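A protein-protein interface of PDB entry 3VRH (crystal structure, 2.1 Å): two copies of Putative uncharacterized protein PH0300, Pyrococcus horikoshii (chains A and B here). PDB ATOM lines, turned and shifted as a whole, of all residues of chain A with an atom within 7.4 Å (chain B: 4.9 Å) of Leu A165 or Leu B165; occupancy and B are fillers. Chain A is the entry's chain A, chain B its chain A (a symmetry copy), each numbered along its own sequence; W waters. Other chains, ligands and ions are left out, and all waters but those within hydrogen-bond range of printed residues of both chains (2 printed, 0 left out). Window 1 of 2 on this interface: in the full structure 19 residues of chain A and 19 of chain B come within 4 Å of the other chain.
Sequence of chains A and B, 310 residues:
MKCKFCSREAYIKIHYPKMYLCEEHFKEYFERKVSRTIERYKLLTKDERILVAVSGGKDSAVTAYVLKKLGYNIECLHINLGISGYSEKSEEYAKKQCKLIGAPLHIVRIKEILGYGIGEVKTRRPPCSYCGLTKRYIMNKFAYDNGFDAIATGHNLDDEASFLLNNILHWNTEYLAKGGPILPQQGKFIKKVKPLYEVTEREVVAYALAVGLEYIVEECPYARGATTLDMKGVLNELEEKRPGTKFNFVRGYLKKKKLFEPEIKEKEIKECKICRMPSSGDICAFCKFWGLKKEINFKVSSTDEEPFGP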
ATOM      1  N   ASP A 159     -10.413  28.541 -20.866  1.00  0.00           N
ATOM      2  CA  ASP A 159      -9.844  27.205 -21.050  1.00  0.00           C
ATOM      3  C   ASP A 159     -10.603  26.141 -20.276  1.00  0.00           C
ATOM      4  O   ASP A 159     -10.969  25.109 -20.845  1.00  0.00           O
ATOM      5  CB  ASP A 159      -8.365  27.180 -20.663  1.00  0.00           C
ATOM      6  CG  ASP A 159      -7.554  28.151 -21.484  1.00  0.00           C
ATOM      7  OD1 ASP A 159      -7.783  28.169 -22.708  1.00  0.00           O
ATOM      8  OD2 ASP A 159      -6.739  28.918 -20.917  1.00  0.00           O
ATOM      9  N   GLU A 160     -10.824  26.375 -18.980  1.00  0.00           N
ATOM     10  CA  GLU A 160     -11.565  25.417 -18.161  1.00  0.00           C
ATOM     11  C   GLU A 160     -12.967  25.161 -18.750  1.00  0.00           C
ATOM     12  O   GLU A 160     -13.394  24.018 -18.864  1.00  0.00           O
ATOM     13  CB  GLU A 160     -11.681  25.895 -16.710  1.00  0.00           C
ATOM     14  CG  GLU A 160     -12.410  24.900 -15.755  1.00  0.00           C
ATOM     15  CD  GLU A 160     -11.528  23.720 -15.307  1.00  0.00           C
ATOM     16  OE1 GLU A 160     -10.558  23.391 -16.023  1.00  0.00           O
ATOM     17  OE2 GLU A 160     -11.798  23.132 -14.227  1.00  0.00           O
ATOM     18  N   ALA A 161     -13.650  26.234 -19.148  1.00  0.00           N
ATOM     19  CA  ALA A 161     -15.008  26.141 -19.673  1.00  0.00           C
ATOM     20  C   ALA A 161     -15.065  25.298 -20.955  1.00  0.00           C
ATOM     21  O   ALA A 161     -15.886  24.382 -21.071  1.00  0.00           O
ATOM     22  CB  ALA A 161     -15.597  27.539 -19.913  1.00  0.00           C
ATOM     23  N   SER A 162     -14.176  25.607 -21.897  1.00  0.00           N
ATOM     24  CA  SER A 162     -14.093  24.887 -23.166  1.00  0.00           C
ATOM     25  C   SER A 162     -13.653  23.427 -23.006  1.00  0.00           C
ATOM     26  O   SER A 162     -14.179  22.541 -23.675  1.00  0.00           O
ATOM     27  CB  SER A 162     -13.160  25.614 -24.136  1.00  0.00           C
ATOM     28  OG  SER A 162     -11.831  25.521 -23.694  1.00  0.00           O
ATOM     29  N   PHE A 163     -12.685  23.191 -22.124  1.00  0.00           N
ATOM     30  CA  PHE A 163     -12.261  21.841 -21.774  1.00  0.00           C
ATOM     31  C   PHE A 163     -13.440  21.088 -21.182  1.00  0.00           C
ATOM     32  O   PHE A 163     -13.690  19.945 -21.553  1.00  0.00           O
ATOM     33  CB  PHE A 163     -11.041  21.883 -20.825  1.00  0.00           C
ATOM     34  CG  PHE A 163     -10.967  20.736 -19.816  1.00  0.00           C
ATOM     35  CD1 PHE A 163     -10.123  19.648 -20.036  1.00  0.00           C
ATOM     36  CD2 PHE A 163     -11.693  20.781 -18.620  1.00  0.00           C
ATOM     37  CE1 PHE A 163     -10.040  18.604 -19.094  1.00  0.00           C
ATOM     38  CE2 PHE A 163     -11.633  19.740 -17.692  1.00  0.00           C
ATOM     39  CZ  PHE A 163     -10.804  18.653 -17.929  1.00  0.00           C
ATOM     40  N   LEU A 164     -14.163  21.734 -20.262  1.00  0.00           N
ATOM     41  CA  LEU A 164     -15.372  21.134 -19.691  1.00  0.00           C
ATOM     42  C   LEU A 164     -16.427  20.781 -20.754  1.00  0.00           C
ATOM     43  O   LEU A 164     -16.929  19.683 -20.763  1.00  0.00           O
ATOM     44  CB  LEU A 164     -16.012  22.018 -18.626  1.00  0.00           C
ATOM     45  CG  LEU A 164     -15.361  22.011 -17.243  1.00  0.00           C
ATOM     46  CD1 LEU A 164     -16.061  22.998 -16.315  1.00  0.00           C
ATOM     47  CD2 LEU A 164     -15.373  20.610 -16.656  1.00  0.00           C
ATOM     48  N   LEU A 165     -16.750  21.718 -21.632  1.00  0.00           N
ATOM     49  CA  LEU A 165     -17.780  21.489 -22.651  1.00  0.00           C
ATOM     50  C   LEU A 165     -17.360  20.363 -23.594  1.00  0.00           C
ATOM     51  O   LEU A 165     -18.139  19.472 -23.916  1.00  0.00           O
ATOM     52  CB  LEU A 165     -18.034  22.772 -23.442  1.00  0.00           C
ATOM     53  CG  LEU A 165     -19.090  22.655 -24.536  1.00  0.00           C
ATOM     54  CD1 LEU A 165     -20.430  22.228 -23.917  1.00  0.00           C
ATOM     55  CD2 LEU A 165     -19.231  23.962 -25.296  1.00  0.00           C
ATOM     56  N   ASN A 166     -16.099  20.396 -24.002  1.00  0.00           N
ATOM     57  CA  ASN A 166     -15.554  19.372 -24.873  1.00  0.00           C
ATOM     58  C   ASN A 166     -15.676  17.998 -24.245  1.00  0.00           C
ATOM     59  O   ASN A 166     -16.220  17.070 -24.850  1.00  0.00           O
ATOM     60  CB  ASN A 166     -14.096  19.686 -25.193  1.00  0.00           C
ATOM     61  CG  ASN A 166     -13.453  18.635 -26.056  1.00  0.00           C
ATOM     62  OD1 ASN A 166     -13.583  18.656 -27.284  1.00  0.00           O
ATOM     63  ND2 ASN A 166     -12.756  17.696 -25.420  1.00  0.00           N
ATOM     64  N   ASN A 167     -15.202  17.867 -23.017  1.00  0.00           N
ATOM     65  CA  ASN A 167     -15.218  16.564 -22.369  1.00  0.00           C
ATOM     66  C   ASN A 167     -16.620  16.048 -22.048  1.00  0.00           C
ATOM     67  O   ASN A 167     -16.824  14.847 -21.945  1.00  0.00           O
ATOM     68  CB  ASN A 167     -14.322  16.554 -21.132  1.00  0.00           C
ATOM     69  CG  ASN A 167     -12.845  16.516 -21.492  1.00  0.00           C
ATOM     70  OD1 ASN A 167     -12.398  15.660 -22.249  1.00  0.00           O
ATOM     71  ND2 ASN A 167     -12.092  17.458 -20.972  1.00  0.00           N
ATOM     72  N   ILE A 168     -17.580  16.953 -21.914  1.00  0.00           N
ATOM     73  CA  ILE A 168     -18.963  16.554 -21.681  1.00  0.00           C
ATOM     74  C   ILE A 168     -19.640  16.084 -22.965  1.00  0.00           C
ATOM     75  O   ILE A 168     -20.391  15.113 -22.958  1.00  0.00           O
ATOM     76  CB  ILE A 168     -19.754  17.699 -21.046  1.00  0.00           C
ATOM     77  CG1 ILE A 168     -19.443  17.757 -19.560  1.00  0.00           C
ATOM     78  CG2 ILE A 168     -21.245  17.512 -21.227  1.00  0.00           C
ATOM     79  CD1 ILE A 168     -19.510  19.133 -18.998  1.00  0.00           C
ATOM     80  N   LEU A 169     -19.388  16.784 -24.060  1.00  0.00           N
ATOM     81  CA  LEU A 169     -19.860  16.328 -25.363  1.00  0.00           C
ATOM     82  C   LEU A 169     -19.388  14.910 -25.672  1.00  0.00           C
ATOM     83  O   LEU A 169     -20.145  14.124 -26.246  1.00  0.00           O
ATOM     84  CB  LEU A 169     -19.395  17.271 -26.469  1.00  0.00           C
ATOM     85  CG  LEU A 169     -20.107  18.620 -26.480  1.00  0.00           C
ATOM     86  CD1 LEU A 169     -19.394  19.577 -27.419  1.00  0.00           C
ATOM     87  CD2 LEU A 169     -21.595  18.448 -26.844  1.00  0.00           C
ATOM     88  N   HIS A 170     -18.140  14.605 -25.290  1.00  0.00           N
ATOM     89  CA  HIS A 170     -17.539  13.291 -25.519  1.00  0.00           C
ATOM     90  C   HIS A 170     -17.774  12.325 -24.384  1.00  0.00           C
ATOM     91  O   HIS A 170     -17.363  11.169 -24.474  1.00  0.00           O
ATOM     92  CB  HIS A 170     -16.027  13.398 -25.702  1.00  0.00           C
ATOM     93  CG  HIS A 170     -15.611  14.029 -26.989  1.00  0.00           C
ATOM     94  ND1 HIS A 170     -14.943  15.233 -27.046  1.00  0.00           N
ATOM     95  CD2 HIS A 170     -15.763  13.621 -28.271  1.00  0.00           C
ATOM     96  CE1 HIS A 170     -14.700  15.542 -28.307  1.00  0.00           C
ATOM     97  NE2 HIS A 170     -15.188  14.581 -29.071  1.00  0.00           N
ATOM     98  N   TRP A 171     -18.407  12.805 -23.313  1.00  0.00           N
ATOM     99  CA  TRP A 171     -18.533  12.050 -22.067  1.00  0.00           C
ATOM    100  C   TRP A 171     -17.211  11.411 -21.589  1.00  0.00           C
ATOM    101  O   TRP A 171     -17.152  10.226 -21.266  1.00  0.00           O
ATOM    102  CB  TRP A 171     -19.708  11.063 -22.144  1.00  0.00           C
ATOM    103  CG  TRP A 171     -21.001  11.834 -22.188  1.00  0.00           C
ATOM    104  CD1 TRP A 171     -21.740  12.166 -23.297  1.00  0.00           C
ATOM    105  CD2 TRP A 171     -21.648  12.453 -21.074  1.00  0.00           C
ATOM    106  NE1 TRP A 171     -22.826  12.939 -22.931  1.00  0.00           N
ATOM    107  CE2 TRP A 171     -22.796  13.118 -21.570  1.00  0.00           C
ATOM    108  CE3 TRP A 171     -21.369  12.509 -19.702  1.00  0.00           C
ATOM    109  CZ2 TRP A 171     -23.663  13.819 -20.738  1.00  0.00           C
ATOM    110  CZ3 TRP A 171     -22.226  13.214 -18.879  1.00  0.00           C
ATOM    111  CH2 TRP A 171     -23.365  13.855 -19.399  1.00  0.00           C
ATOM    112  N   LEU A 176     -13.181  14.417 -16.573  1.00  0.00           N
ATOM    113  CA  LEU A 176     -14.103  15.272 -15.823  1.00  0.00           C
ATOM    114  C   LEU A 176     -13.907  15.176 -14.315  1.00  0.00           C
ATOM    115  O   LEU A 176     -14.294  16.086 -13.568  1.00  0.00           O
ATOM    116  CB  LEU A 176     -15.567  14.941 -16.165  1.00  0.00           C
ATOM    117  CG  LEU A 176     -16.056  15.347 -17.559  1.00  0.00           C
ATOM    118  CD1 LEU A 176     -17.449  14.789 -17.806  1.00  0.00           C
ATOM    119  CD2 LEU A 176     -16.029  16.855 -17.718  1.00  0.00           C
ATOM    120  N   ASP A 230     -13.416  25.765 -31.258  1.00  0.00           N
ATOM    121  CA  ASP A 230     -14.835  25.582 -31.551  1.00  0.00           C
ATOM    122  C   ASP A 230     -15.640  25.795 -30.276  1.00  0.00           C
ATOM    123  O   ASP A 230     -16.651  26.500 -30.288  1.00  0.00           O
ATOM    124  CB  ASP A 230     -15.124  24.181 -32.120  1.00  0.00           C
ATOM    125  CG  ASP A 230     -14.784  24.060 -33.598  1.00  0.00           C
ATOM    126  OD1 ASP A 230     -14.477  25.093 -34.231  1.00  0.00           O
ATOM    127  OD2 ASP A 230     -14.841  22.930 -34.130  1.00  0.00           O
ATOM    128  N   MET A 231     -15.184  25.184 -29.179  1.00  0.00           N
ATOM    129  CA  MET A 231     -15.873  25.295 -27.893  1.00  0.00           C
ATOM    130  C   MET A 231     -15.843  26.723 -27.385  1.00  0.00           C
ATOM    131  O   MET A 231     -16.837  27.213 -26.861  1.00  0.00           O
ATOM    132  CB  MET A 231     -15.259  24.361 -26.852  1.00  0.00           C
ATOM    133  CG  MET A 231     -15.172  22.906 -27.283  1.00  0.00           C
ATOM    134  SD  MET A 231     -16.762  22.032 -27.376  1.00  0.00           S
ATOM    135  CE  MET A 231     -17.202  22.223 -29.106  1.00  0.00           C
ATOM    136  N   LYS A 232     -14.706  27.393 -27.536  1.00  0.00           N
ATOM    137  CA  LYS A 232     -14.591  28.754 -27.039  1.00  0.00           C
ATOM    138  C   LYS A 232     -15.547  29.674 -27.795  1.00  0.00           C
ATOM    139  O   LYS A 232     -16.144  30.567 -27.193  1.00  0.00           O
ATOM    140  CB  LYS A 232     -13.145  29.273 -27.103  1.00  0.00           C
ATOM    141  CG  LYS A 232     -12.225  28.677 -26.038  1.00  0.00           C
ATOM    142  CD  LYS A 232     -10.776  29.078 -26.230  1.00  0.00           C
ATOM    143  CE  LYS A 232      -9.923  28.617 -25.032  1.00  0.00           C
ATOM    144  NZ  LYS A 232      -8.606  29.347 -24.902  1.00  0.00           N
ATOM    145  N   VAL A 234     -18.418  28.821 -29.424  1.00  0.00           N
ATOM    146  CA  VAL A 234     -19.733  28.470 -28.906  1.00  0.00           C
ATOM    147  C   VAL A 234     -19.991  29.148 -27.555  1.00  0.00           C
ATOM    148  O   VAL A 234     -21.037  29.763 -27.344  1.00  0.00           O
ATOM    149  CB  VAL A 234     -19.835  26.949 -28.735  1.00  0.00           C
ATOM    150  CG1 VAL A 234     -20.946  26.587 -27.798  1.00  0.00           C
ATOM    151  CG2 VAL A 234     -20.024  26.283 -30.081  1.00  0.00           C
ATOM    152  N   LEU A 235     -19.022  29.048 -26.648  1.00  0.00           N
ATOM    153  CA  LEU A 235     -19.189  29.605 -25.311  1.00  0.00           C
ATOM    154  C   LEU A 235     -19.233  31.128 -25.343  1.00  0.00           C
ATOM    155  O   LEU A 235     -19.957  31.745 -24.568  1.00  0.00           O
ATOM    156  CB  LEU A 235     -18.080  29.120 -24.378  1.00  0.00           C
ATOM    157  CG  LEU A 235     -18.137  27.633 -24.043  1.00  0.00           C
ATOM    158  CD1 LEU A 235     -16.817  27.194 -23.464  1.00  0.00           C
ATOM    159  CD2 LEU A 235     -19.245  27.378 -23.055  1.00  0.00           C
ATOM    160  N   LEU A 238     -22.781  31.944 -26.562  1.00  0.00           N
ATOM    161  CA  LEU A 238     -23.675  31.855 -25.403  1.00  0.00           C
ATOM    162  C   LEU A 238     -23.490  32.978 -24.376  1.00  0.00           C
ATOM    163  O   LEU A 238     -24.473  33.486 -23.816  1.00  0.00           O
ATOM    164  CB  LEU A 238     -23.526  30.499 -24.710  1.00  0.00           C
ATOM    165  CG  LEU A 238     -24.006  29.315 -25.529  1.00  0.00           C
ATOM    166  CD1 LEU A 238     -23.843  28.037 -24.741  1.00  0.00           C
ATOM    167  CD2 LEU A 238     -25.466  29.512 -25.924  1.00  0.00           C
ATOM    168  N   PHE A 249     -21.342  28.008 -15.404  1.00  0.00           N
ATOM    169  CA  PHE A 249     -20.985  26.649 -15.812  1.00  0.00           C
ATOM    170  C   PHE A 249     -19.861  26.058 -14.966  1.00  0.00           C
ATOM    171  O   PHE A 249     -19.963  24.917 -14.483  1.00  0.00           O
ATOM    172  CB  PHE A 249     -20.572  26.676 -17.287  1.00  0.00           C
ATOM    173  CG  PHE A 249     -20.323  25.324 -17.887  1.00  0.00           C
ATOM    174  CD1 PHE A 249     -21.139  24.235 -17.564  1.00  0.00           C
ATOM    175  CD2 PHE A 249     -19.294  25.143 -18.821  1.00  0.00           C
ATOM    176  CE1 PHE A 249     -20.926  23.006 -18.145  1.00  0.00           C
ATOM    177  CE2 PHE A 249     -19.071  23.889 -19.406  1.00  0.00           C
ATOM    178  CZ  PHE A 249     -19.897  22.829 -19.069  1.00  0.00           C
ATOM    179  N   ALA B 161     -30.919  16.364 -27.002  1.00  0.00           N
ATOM    180  CA  ALA B 161     -29.585  16.952 -27.047  1.00  0.00           C
ATOM    181  C   ALA B 161     -29.554  18.341 -26.393  1.00  0.00           C
ATOM    182  O   ALA B 161     -28.702  18.618 -25.542  1.00  0.00           O
ATOM    183  CB  ALA B 161     -29.067  17.019 -28.491  1.00  0.00           C
ATOM    184  N   SER B 162     -30.500  19.192 -26.786  1.00  0.00           N
ATOM    185  CA  SER B 162     -30.613  20.545 -26.243  1.00  0.00           C
ATOM    186  C   SER B 162     -30.984  20.572 -24.755  1.00  0.00           C
ATOM    187  O   SER B 162     -30.454  21.380 -23.997  1.00  0.00           O
ATOM    188  CB  SER B 162     -31.621  21.364 -27.052  1.00  0.00           C
ATOM    189  OG  SER B 162     -32.923  20.885 -26.834  1.00  0.00           O
ATOM    190  N   PHE B 163     -31.898  19.692 -24.355  1.00  0.00           N
ATOM    191  CA  PHE B 163     -32.247  19.517 -22.950  1.00  0.00           C
ATOM    192  C   PHE B 163     -31.011  19.085 -22.181  1.00  0.00           C
ATOM    193  O   PHE B 163     -30.732  19.622 -21.113  1.00  0.00           O
ATOM    194  CB  PHE B 163     -33.421  18.521 -22.803  1.00  0.00           C
ATOM    195  CG  PHE B 163     -33.398  17.680 -21.526  1.00  0.00           C
ATOM    196  CD1 PHE B 163     -34.205  18.014 -20.438  1.00  0.00           C
ATOM    197  CD2 PHE B 163     -32.618  16.521 -21.440  1.00  0.00           C
ATOM    198  CE1 PHE B 163     -34.199  17.225 -19.272  1.00  0.00           C
ATOM    199  CE2 PHE B 163     -32.590  15.746 -20.279  1.00  0.00           C
ATOM    200  CZ  PHE B 163     -33.383  16.096 -19.197  1.00  0.00           C
ATOM    201  N   LEU B 164     -30.272  18.115 -22.728  1.00  0.00           N
ATOM    202  CA  LEU B 164     -29.013  17.685 -22.114  1.00  0.00           C
ATOM    203  C   LEU B 164     -27.997  18.830 -21.961  1.00  0.00           C
ATOM    204  O   LEU B 164     -27.449  19.013 -20.901  1.00  0.00           O
ATOM    205  CB  LEU B 164     -28.360  16.534 -22.873  1.00  0.00           C
ATOM    206  CG  LEU B 164     -28.943  15.140 -22.644  1.00  0.00           C
ATOM    207  CD1 LEU B 164     -28.241  14.113 -23.527  1.00  0.00           C
ATOM    208  CD2 LEU B 164     -28.844  14.756 -21.178  1.00  0.00           C
ATOM    209  N   LEU B 165     -27.755  19.581 -23.025  1.00  0.00           N
ATOM    210  CA  LEU B 165     -26.767  20.664 -22.988  1.00  0.00           C
ATOM    211  C   LEU B 165     -27.185  21.737 -21.983  1.00  0.00           C
ATOM    212  O   LEU B 165     -26.385  22.212 -21.184  1.00  0.00           O
ATOM    213  CB  LEU B 165     -26.605  21.278 -24.379  1.00  0.00           C
ATOM    214  CG  LEU B 165     -25.599  22.421 -24.465  1.00  0.00           C
ATOM    215  CD1 LEU B 165     -24.215  21.924 -24.021  1.00  0.00           C
ATOM    216  CD2 LEU B 165     -25.549  22.996 -25.868  1.00  0.00           C
ATOM    217  N   ASN B 166     -28.464  22.083 -22.012  1.00  0.00           N
ATOM    218  CA  ASN B 166     -29.007  23.065 -21.093  1.00  0.00           C
ATOM    219  C   ASN B 166     -28.797  22.641 -19.653  1.00  0.00           C
ATOM    220  O   ASN B 166     -28.245  23.391 -18.844  1.00  0.00           O
ATOM    221  CB  ASN B 166     -30.491  23.277 -21.377  1.00  0.00           C
ATOM    222  CG  ASN B 166     -31.130  24.250 -20.425  1.00  0.00           C
ATOM    223  OD1 ASN B 166     -31.060  25.467 -20.621  1.00  0.00           O
ATOM    224  ND2 ASN B 166     -31.756  23.723 -19.376  1.00  0.00           N
ATOM    225  N   ASN B 167     -29.205  21.424 -19.331  1.00  0.00           N
ATOM    226  CA  ASN B 167     -29.104  20.966 -17.954  1.00  0.00           C
ATOM    227  C   ASN B 167     -27.668  20.779 -17.466  1.00  0.00           C
ATOM    228  O   ASN B 167     -27.410  20.853 -16.274  1.00  0.00           O
ATOM    229  CB  ASN B 167     -29.939  19.706 -17.731  1.00  0.00           C
ATOM    230  CG  ASN B 167     -31.428  20.006 -17.671  1.00  0.00           C
ATOM    231  OD1 ASN B 167     -31.874  20.855 -16.907  1.00  0.00           O
ATOM    232  ND2 ASN B 167     -32.194  19.328 -18.496  1.00  0.00           N
ATOM    233  N   ILE B 168     -26.742  20.560 -18.390  1.00  0.00           N
ATOM    234  CA  ILE B 168     -25.333  20.443 -18.030  1.00  0.00           C
ATOM    235  C   ILE B 168     -24.700  21.808 -17.773  1.00  0.00           C
ATOM    236  O   ILE B 168     -23.909  21.968 -16.848  1.00  0.00           O
ATOM    237  CB  ILE B 168     -24.561  19.688 -19.113  1.00  0.00           C
ATOM    238  CG1 ILE B 168     -24.802  18.197 -18.951  1.00  0.00           C
ATOM    239  CG2 ILE B 168     -23.075  19.956 -19.024  1.00  0.00           C
ATOM    240  CD1 ILE B 168     -24.766  17.452 -20.238  1.00  0.00           C
ATOM    241  N   LEU B 169     -25.033  22.782 -18.605  1.00  0.00           N
ATOM    242  CA  LEU B 169     -24.606  24.155 -18.355  1.00  0.00           C
ATOM    243  C   LEU B 169     -25.033  24.639 -16.973  1.00  0.00           C
ATOM    244  O   LEU B 169     -24.272  25.348 -16.310  1.00  0.00           O
ATOM    245  CB  LEU B 169     -25.162  25.098 -19.418  1.00  0.00           C
ATOM    246  CG  LEU B 169     -24.509  24.950 -20.789  1.00  0.00           C
ATOM    247  CD1 LEU B 169     -25.306  25.716 -21.831  1.00  0.00           C
ATOM    248  CD2 LEU B 169     -23.035  25.396 -20.740  1.00  0.00           C
ATOM    249  N   MET B 231     -29.826  26.498 -27.417  1.00  0.00           N
ATOM    250  CA  MET B 231     -29.081  25.239 -27.383  1.00  0.00           C
ATOM    251  C   MET B 231     -29.147  24.536 -28.724  1.00  0.00           C
ATOM    252  O   MET B 231     -28.150  23.991 -29.185  1.00  0.00           O
ATOM    253  CB  MET B 231     -29.605  24.314 -26.286  1.00  0.00           C
ATOM    254  CG  MET B 231     -29.651  24.940 -24.902  1.00  0.00           C
ATOM    255  SD  MET B 231     -28.033  25.220 -24.127  1.00  0.00           S
ATOM    256  CE  MET B 231     -27.685  26.923 -24.575  1.00  0.00           C
ATOM    257  N   VAL B 234     -26.763  26.368 -31.205  1.00  0.00           N
ATOM    258  CA  VAL B 234     -25.411  25.959 -30.849  1.00  0.00           C
ATOM    259  C   VAL B 234     -25.117  24.539 -31.347  1.00  0.00           C
ATOM    260  O   VAL B 234     -24.088  24.288 -31.977  1.00  0.00           O
ATOM    261  CB  VAL B 234     -25.238  26.007 -29.326  1.00  0.00           C
ATOM    262  CG1 VAL B 234     -24.068  25.177 -28.893  1.00  0.00           C
ATOM    263  CG2 VAL B 234     -25.086  27.439 -28.861  1.00  0.00           C
ATOM    264  N   LEU B 235     -26.036  23.615 -31.076  1.00  0.00           N
ATOM    265  CA  LEU B 235     -25.829  22.221 -31.451  1.00  0.00           C
ATOM    266  C   LEU B 235     -25.849  22.042 -32.964  1.00  0.00           C
ATOM    267  O   LEU B 235     -25.116  21.220 -33.503  1.00  0.00           O
ATOM    268  CB  LEU B 235     -26.870  21.319 -30.790  1.00  0.00           C
ATOM    269  CG  LEU B 235     -26.734  21.198 -29.275  1.00  0.00           C
ATOM    270  CD1 LEU B 235     -28.006  20.632 -28.698  1.00  0.00           C
ATOM    271  CD2 LEU B 235     -25.571  20.303 -28.940  1.00  0.00           C
ATOM    272  N   PHE B 249     -23.136  12.733 -28.612  1.00  0.00           N
ATOM    273  CA  PHE B 249     -23.455  13.312 -27.306  1.00  0.00           C
ATOM    274  C   PHE B 249     -24.512  12.511 -26.551  1.00  0.00           C
ATOM    275  O   PHE B 249     -24.339  12.196 -25.360  1.00  0.00           O
ATOM    276  CB  PHE B 249     -23.940  14.751 -27.516  1.00  0.00           C
ATOM    277  CG  PHE B 249     -24.160  15.522 -26.249  1.00  0.00           C
ATOM    278  CD1 PHE B 249     -23.285  15.389 -25.167  1.00  0.00           C
ATOM    279  CD2 PHE B 249     -25.225  16.428 -26.149  1.00  0.00           C
ATOM    280  CE1 PHE B 249     -23.474  16.126 -24.020  1.00  0.00           C
ATOM    281  CE2 PHE B 249     -25.423  17.173 -24.978  1.00  0.00           C
ATOM    282  CZ  PHE B 249     -24.538  17.022 -23.923  1.00  0.00           C
HETATM  283  O   HOH W   1     -24.311  28.329 -17.183  1.00  0.00           O
HETATM  284  O   HOH W   2     -20.272  14.573 -29.317  1.00  0.00           O
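Water W2 lies within hydrogen-bond range of O of Leu A169 (3.1 Å) and N of Phe B249 (3.5 Å). Water W1 bridges the backbone carbonyl oxygen of Leu B169 and the backbone NH of Phe A249.
Of the printed residues of chain B, Trp A171 touches Ile B168 (3.8 Å) and Phe B249 (3.0 Å). Printed residues of chain B within 4 Å of Phe A249: Ile B168 and Leu B169. Printed residues of chain B within 4 Å of Ile A168: Ile B168 (3.7 Å) and Phe B249 (3.4 Å). Of the printed residues of chain A, Met B231 touches Leu A238 (3.7 Å). Of the printed residues of chain A, Val B234 touches Val A234 (3.6 Å) and Leu A238 (3.6 Å). The nearest residue of chain A that does not touch Leu B165 is Leu A169 (5.2 Å). The nearest printed residue of chain A that does not touch Phe B249 is His A170 (5.2 Å).
Of the 21 printed residues of chain A, 7 touch a printed residue of chain B. Hydrophobic or aromatic side chains of chain A within 4 Å of the printed part of chain B: Leu A165, Ile A168, Leu A169, Trp A171, Val A234, Leu A238 and Phe A249. Of the 13 printed residues of chain B, 6 touch a printed residue of chain A. Among the printed residues, 12 pairs touch across the chains. Among the printed residues, no Asp or Glu carboxylate lies within 4 Å of a Lys or Arg side-chain nitrogen of the other chain.
The backbone carbonyl oxygen (O) of Ile A168 sits close to the indole nitrogen (NE1) of Trp A171, 3.3 Å away.
CD1 of Leu A165 touches CD1 of Leu B165, at 3.8 Å. Phe B249 touches Ile A168. Phe B249 touches Leu A169. CD1 of Ile B168 touches CZ2 of Trp A171 (3.8 Å). CG1 of Val A234 touches CG1 of Val B234, 3.6 Å away. CD1 of Leu A238 touches CD1 of Leu B169 (3.999 Å). Leu A238 touches Met B231. CD2 of Leu A238 touches CG2 of Val B234, 3.6 Å away. O of Ile B168 touches CE1 of Phe A249, 3.4 Å away. O of Leu B169 touches CD1 of Phe A249, at 3.6 Å.
The indole nitrogen (NE1) of Trp A171 sits at hydrogen-bond distance from the backbone carbonyl oxygen (O) of Phe B249.
Leu A165 touches its own counterpart, Leu B165. Ile A168 touches its own counterpart, Ile B168. Ile A168 touches Phe B249, and with the chains exchanged Phe A249 touches Ile B168. Val A234 touches its own counterpart, Val B234.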
